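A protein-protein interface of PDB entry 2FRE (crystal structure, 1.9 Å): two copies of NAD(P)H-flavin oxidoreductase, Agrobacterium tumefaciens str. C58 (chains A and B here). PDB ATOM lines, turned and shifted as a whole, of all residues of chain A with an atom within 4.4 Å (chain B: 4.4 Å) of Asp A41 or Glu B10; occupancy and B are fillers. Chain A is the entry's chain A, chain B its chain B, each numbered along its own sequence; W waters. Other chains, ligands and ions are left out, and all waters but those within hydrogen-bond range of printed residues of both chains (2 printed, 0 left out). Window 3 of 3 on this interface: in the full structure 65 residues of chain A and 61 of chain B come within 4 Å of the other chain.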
ATOM      1  N   LEU A  37       2.133 -10.749  -9.253  1.00  0.00           N
ATOM      2  CA  LEU A  37       3.580 -10.616  -9.192  1.00  0.00           C
ATOM      3  C   LEU A  37       3.998  -9.177  -8.822  1.00  0.00           C
ATOM      4  O   LEU A  37       4.919  -8.969  -8.012  1.00  0.00           O
ATOM      5  CB  LEU A  37       4.212 -11.123 -10.507  1.00  0.00           C
ATOM      6  CG  LEU A  37       4.145 -12.657 -10.687  1.00  0.00           C
ATOM      7  CD1 LEU A  37       4.602 -13.073 -12.067  1.00  0.00           C
ATOM      8  CD2 LEU A  37       4.978 -13.407  -9.642  1.00  0.00           C
ATOM      9  N   THR A  38       3.280  -8.188  -9.345  1.00  0.00           N
ATOM     10  CA  THR A  38       3.504  -6.790  -8.965  1.00  0.00           C
ATOM     11  C   THR A  38       3.272  -6.588  -7.464  1.00  0.00           C
ATOM     12  O   THR A  38       4.096  -5.970  -6.760  1.00  0.00           O
ATOM     13  CB  THR A  38       2.617  -5.838  -9.807  1.00  0.00           C
ATOM     14  OG1 THR A  38       2.851  -6.077 -11.197  1.00  0.00           O
ATOM     15  CG2 THR A  38       2.945  -4.381  -9.525  1.00  0.00           C
ATOM     16  N   ILE A  39       2.166  -7.151  -6.977  1.00  0.00           N
ATOM     17  CA  ILE A  39       1.804  -7.094  -5.555  1.00  0.00           C
ATOM     18  C   ILE A  39       2.887  -7.691  -4.675  1.00  0.00           C
ATOM     19  O   ILE A  39       3.282  -7.079  -3.696  1.00  0.00           O
ATOM     20  CB  ILE A  39       0.443  -7.784  -5.298  1.00  0.00           C
ATOM     21  CG1 ILE A  39      -0.674  -6.927  -5.920  1.00  0.00           C
ATOM     22  CG2 ILE A  39       0.204  -7.988  -3.790  1.00  0.00           C
ATOM     23  CD1 ILE A  39      -2.013  -7.586  -5.948  1.00  0.00           C
ATOM     24  N   LEU A  40       3.371  -8.877  -5.030  1.00  0.00           N
ATOM     25  CA  LEU A  40       4.419  -9.522  -4.254  1.00  0.00           C
ATOM     26  C   LEU A  40       5.777  -8.839  -4.444  1.00  0.00           C
ATOM     27  O   LEU A  40       6.594  -8.829  -3.535  1.00  0.00           O
ATOM     28  CB  LEU A  40       4.477 -11.027  -4.570  1.00  0.00           C
ATOM     29  CG  LEU A  40       3.227 -11.830  -4.188  1.00  0.00           C
ATOM     30  CD1 LEU A  40       3.398 -13.335  -4.524  1.00  0.00           C
ATOM     31  CD2 LEU A  40       2.833 -11.656  -2.752  1.00  0.00           C
ATOM     32  N   ASP A  41       5.998  -8.224  -5.609  1.00  0.00           N
ATOM     33  CA  ASP A  41       7.211  -7.444  -5.860  1.00  0.00           C
ATOM     34  C   ASP A  41       7.268  -6.244  -4.903  1.00  0.00           C
ATOM     35  O   ASP A  41       8.273  -6.010  -4.243  1.00  0.00           O
ATOM     36  CB  ASP A  41       7.254  -6.978  -7.333  1.00  0.00           C
ATOM     37  CG  ASP A  41       8.628  -6.540  -7.775  1.00  0.00           C
ATOM     38  OD1 ASP A  41       9.610  -6.679  -7.007  1.00  0.00           O
ATOM     39  OD2 ASP A  41       8.735  -6.071  -8.916  1.00  0.00           O
ATOM     40  N   ALA A  42       6.160  -5.523  -4.771  1.00  0.00           N
ATOM     41  CA  ALA A  42       6.094  -4.414  -3.809  1.00  0.00           C
ATOM     42  C   ALA A  42       6.355  -4.882  -2.368  1.00  0.00           C
ATOM     43  O   ALA A  42       7.120  -4.249  -1.613  1.00  0.00           O
ATOM     44  CB  ALA A  42       4.733  -3.691  -3.924  1.00  0.00           C
ATOM     45  N   ALA A  43       5.719  -5.991  -1.990  1.00  0.00           N
ATOM     46  CA  ALA A  43       5.910  -6.606  -0.683  1.00  0.00           C
ATOM     47  C   ALA A  43       7.398  -6.908  -0.380  1.00  0.00           C
ATOM     48  O   ALA A  43       7.881  -6.617   0.714  1.00  0.00           O
ATOM     49  CB  ALA A  43       5.045  -7.893  -0.569  1.00  0.00           C
ATOM     50  N   HIS A  44       8.113  -7.435  -1.363  1.00  0.00           N
ATOM     51  CA  HIS A  44       9.514  -7.840  -1.206  1.00  0.00           C
ATOM     52  C   HIS A  44      10.490  -6.662  -1.202  1.00  0.00           C
ATOM     53  O   HIS A  44      11.684  -6.846  -0.916  1.00  0.00           O
ATOM     54  CB  HIS A  44       9.879  -8.922  -2.262  1.00  0.00           C
ATOM     55  CG  HIS A  44      10.773  -8.465  -3.378  1.00  0.00           C
ATOM     56  ND1 HIS A  44      11.977  -9.082  -3.659  1.00  0.00           N
ATOM     57  CD2 HIS A  44      10.633  -7.487  -4.300  1.00  0.00           C
ATOM     58  CE1 HIS A  44      12.538  -8.498  -4.704  1.00  0.00           C
ATOM     59  NE2 HIS A  44      11.752  -7.516  -5.103  1.00  0.00           N
ATOM     60  N   TRP A  45       9.988  -5.468  -1.532  1.00  0.00           N
ATOM     61  CA  TRP A  45      10.754  -4.223  -1.379  1.00  0.00           C
ATOM     62  C   TRP A  45      10.697  -3.613   0.030  1.00  0.00           C
ATOM     63  O   TRP A  45      11.250  -2.530   0.271  1.00  0.00           O
ATOM     64  CB  TRP A  45      10.350  -3.182  -2.438  1.00  0.00           C
ATOM     65  CG  TRP A  45      11.085  -3.377  -3.677  1.00  0.00           C
ATOM     66  CD1 TRP A  45      10.624  -3.917  -4.841  1.00  0.00           C
ATOM     67  CD2 TRP A  45      12.456  -3.066  -3.892  1.00  0.00           C
ATOM     68  NE1 TRP A  45      11.623  -3.952  -5.773  1.00  0.00           N
ATOM     69  CE2 TRP A  45      12.765  -3.440  -5.214  1.00  0.00           C
ATOM     70  CE3 TRP A  45      13.457  -2.494  -3.094  1.00  0.00           C
ATOM     71  CZ2 TRP A  45      14.033  -3.269  -5.754  1.00  0.00           C
ATOM     72  CZ3 TRP A  45      14.723  -2.338  -3.631  1.00  0.00           C
ATOM     73  CH2 TRP A  45      14.994  -2.717  -4.950  1.00  0.00           C
ATOM     74  N   MET B   1       8.035  -3.071 -15.652  1.00  0.00           N
ATOM     75  CA  MET B   1       9.159  -2.879 -14.683  1.00  0.00           C
ATOM     76  C   MET B   1       9.447  -1.394 -14.374  1.00  0.00           C
ATOM     77  O   MET B   1       9.362  -0.530 -15.248  1.00  0.00           O
ATOM     78  CB  MET B   1      10.402  -3.581 -15.205  1.00  0.00           C
ATOM     79  CG  MET B   1      11.028  -2.912 -16.374  1.00  0.00           C
ATOM     80  SD  MET B   1      12.781  -2.173 -15.928  1.00  0.00           S
ATOM     81  CE  MET B   1      12.456  -1.251 -14.348  1.00  0.00           C
ATOM     82  N   GLN B   8      15.767  -0.891  -9.387  1.00  0.00           N
ATOM     83  CA  GLN B   8      15.029  -1.411 -10.518  1.00  0.00           C
ATOM     84  C   GLN B   8      14.158  -2.569 -10.082  1.00  0.00           C
ATOM     85  O   GLN B   8      14.661  -3.526  -9.502  1.00  0.00           O
ATOM     86  CB  GLN B   8      15.989  -1.850 -11.632  1.00  0.00           C
ATOM     87  CG  GLN B   8      15.266  -2.512 -12.775  1.00  0.00           C
ATOM     88  CD  GLN B   8      16.062  -2.562 -14.060  1.00  0.00           C
ATOM     89  OE1 GLN B   8      16.458  -1.523 -14.619  1.00  0.00           O
ATOM     90  NE2 GLN B   8      16.288  -3.776 -14.556  1.00  0.00           N
ATOM     91  N   SER B   9      12.859  -2.487 -10.362  1.00  0.00           N
ATOM     92  CA  SER B   9      11.938  -3.568 -10.027  1.00  0.00           C
ATOM     93  C   SER B   9      11.755  -4.516 -11.206  1.00  0.00           C
ATOM     94  O   SER B   9      11.945  -4.126 -12.355  1.00  0.00           O
ATOM     95  CB  SER B   9      10.571  -3.015  -9.629  1.00  0.00           C
ATOM     96  OG  SER B   9       9.827  -2.646 -10.791  1.00  0.00           O
ATOM     97  N   GLU B  10      11.358  -5.751 -10.920  1.00  0.00           N
ATOM     98  CA  GLU B  10      11.088  -6.729 -11.967  1.00  0.00           C
ATOM     99  C   GLU B  10       9.695  -6.509 -12.560  1.00  0.00           C
ATOM    100  O   GLU B  10       9.463  -6.767 -13.739  1.00  0.00           O
ATOM    101  CB  GLU B  10      11.193  -8.148 -11.408  1.00  0.00           C
ATOM    102  CG  GLU B  10      12.611  -8.564 -11.018  1.00  0.00           C
ATOM    103  CD  GLU B  10      12.647  -9.832 -10.161  1.00  0.00           C
ATOM    104  OE1 GLU B  10      12.588 -10.955 -10.716  1.00  0.00           O
ATOM    105  OE2 GLU B  10      12.764  -9.710  -8.932  1.00  0.00           O
ATOM    106  N   TYR B  11       8.767  -6.048 -11.726  1.00  0.00           N
ATOM    107  CA  TYR B  11       7.373  -5.850 -12.123  1.00  0.00           C
ATOM    108  C   TYR B  11       6.978  -4.404 -11.899  1.00  0.00           C
ATOM    109  O   TYR B  11       7.668  -3.701 -11.175  1.00  0.00           O
ATOM    110  CB  TYR B  11       6.486  -6.838 -11.358  1.00  0.00           C
ATOM    111  CG  TYR B  11       6.872  -8.265 -11.684  1.00  0.00           C
ATOM    112  CD1 TYR B  11       6.344  -8.910 -12.800  1.00  0.00           C
ATOM    113  CD2 TYR B  11       7.794  -8.950 -10.905  1.00  0.00           C
ATOM    114  CE1 TYR B  11       6.711 -10.205 -13.114  1.00  0.00           C
ATOM    115  CE2 TYR B  11       8.165 -10.234 -11.208  1.00  0.00           C
ATOM    116  CZ  TYR B  11       7.624 -10.861 -12.317  1.00  0.00           C
ATOM    117  OH  TYR B  11       8.004 -12.150 -12.632  1.00  0.00           O
ATOM    118  N   VAL B  13       5.804  -2.061 -10.153  1.00  0.00           N
ATOM    119  CA  VAL B  13       5.374  -1.582  -8.833  1.00  0.00           C
ATOM    120  C   VAL B  13       5.216  -0.053  -8.868  1.00  0.00           C
ATOM    121  O   VAL B  13       5.848   0.647  -9.686  1.00  0.00           O
ATOM    122  CB  VAL B  13       6.349  -1.993  -7.665  1.00  0.00           C
ATOM    123  CG1 VAL B  13       6.532  -3.500  -7.568  1.00  0.00           C
ATOM    124  CG2 VAL B  13       7.721  -1.304  -7.769  1.00  0.00           C
ATOM    125  N   PRO B 185      15.949 -11.577  -6.109  1.00  0.00           N
ATOM    126  CA  PRO B 185      14.868 -11.716  -7.107  1.00  0.00           C
ATOM    127  C   PRO B 185      13.559 -12.153  -6.460  1.00  0.00           C
ATOM    128  O   PRO B 185      13.570 -12.919  -5.491  1.00  0.00           O
ATOM    129  CB  PRO B 185      15.406 -12.804  -8.056  1.00  0.00           C
ATOM    130  CG  PRO B 185      16.893 -12.701  -7.940  1.00  0.00           C
ATOM    131  CD  PRO B 185      17.135 -12.363  -6.480  1.00  0.00           C
ATOM    132  N   LEU B 186      12.435 -11.655  -6.967  1.00  0.00           N
ATOM    133  CA  LEU B 186      11.134 -12.029  -6.438  1.00  0.00           C
ATOM    134  C   LEU B 186      10.969 -13.551  -6.326  1.00  0.00           C
ATOM    135  O   LEU B 186      10.468 -14.042  -5.319  1.00  0.00           O
ATOM    136  CB  LEU B 186      10.019 -11.455  -7.323  1.00  0.00           C
ATOM    137  CG  LEU B 186       8.577 -11.691  -6.863  1.00  0.00           C
ATOM    138  CD1 LEU B 186       8.420 -11.389  -5.400  1.00  0.00           C
ATOM    139  CD2 LEU B 186       7.596 -10.861  -7.722  1.00  0.00           C
HETATM  140  O   HOH W   1      14.250  -7.324  -6.946  1.00  0.00           O
HETATM  141  O   HOH W   2      11.939  -6.601  -8.127  1.00  0.00           O
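OD2 of Asp A41 lies within hydrogen-bond range of N of Tyr B11, at 2.8 Å.
The side-chain carboxylate of Asp A41 lies within hydrogen-bond range of the backbone NH of Glu B10 (3.3 Å).
OE2 of Glu B10 sits at hydrogen-bond distance from N of Leu B186 (2.8 Å).
The side-chain hydroxyl (OG) of Ser B9 is in hydrogen-bond range of the backbone carbonyl oxygen (O) of Tyr B11 (2.4 Å).
A ring nitrogen (NE2) of His A44 is in hydrogen-bond range of the side-chain carboxylate of Asp A41 (3.0 Å).
Of the printed residues of chain B, Leu A37 touches Tyr B11 and Leu B186.
Of chain B, only Ser B9 (3.6 Å), Glu B10 (3.3 Å), Tyr B11 (2.8 Å), Val B13 (3.6 Å) and Leu B186 (3.7 Å) come within 4 Å of Asp A41.
Of the printed residues of chain B, His A44 touches Leu B186.
Printed residues of chain B within 4 Å of Trp A45: Gln B8 (3.8 Å).
Met B1 touches none of the printed residues of chain A.
Of the printed residues of chain A, Ser B9 touches Asp A41.
Of the printed residues of chain A, Leu B186 touches Leu A37, Leu A40, Asp A41 and His A44.
The nearest printed residue of chain B that does not touch Asp A41 is Gln B8 (6.5 Å).
Along chain B the printed residues that touch a printed residue of chain A span positions 8 to 186.
Hydrophobic or aromatic side chains of chain A within 4 Å of the printed part of chain B: Leu A37, His A44 and Trp A45.
Among the printed residues, 13 pairs touch across the chains.
Among the printed residues, no Asp or Glu carboxylate lies within 4 Å of a Lys or Arg side-chain nitrogen of the other chain.
No position is printed for both chains.
Of the 13 pairs that touch across the chains among the printed residues, none has its exchanged pair printed and touching as well.
Water W2 lies within hydrogen-bond range of OD1 of Asp A41, N of Glu B10 and NE2 of His A44.
Water W1 lies within hydrogen-bond range of a ring nitrogen (NE2) of His A44 (3.1 Å) and the side-chain carboxylate (OE2) of Glu B10 (3.4 Å).
Leu A37 touches Tyr B11 (CD1 to OH, 3.6 Å).
Leu A37 touches Leu B186.
Tyr B11 touches Thr A38.
Thr A38 touches Val B13 (O to CG1, 3.6 Å).
Leu A40 touches Leu B186 (O to CD1, 3.7 Å).
CB of Ser B9 touches OD2 of Asp A41 (3.6 Å).
CB of Asp A41 touches CG1 of Val B13, 3.6 Å away.
N of Asp A41 touches CD2 of Leu B186 (3.7 Å).
CE1 of His A44 touches N of Leu B186, at 3.9 Å.
Trp A45 touches Gln B8.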
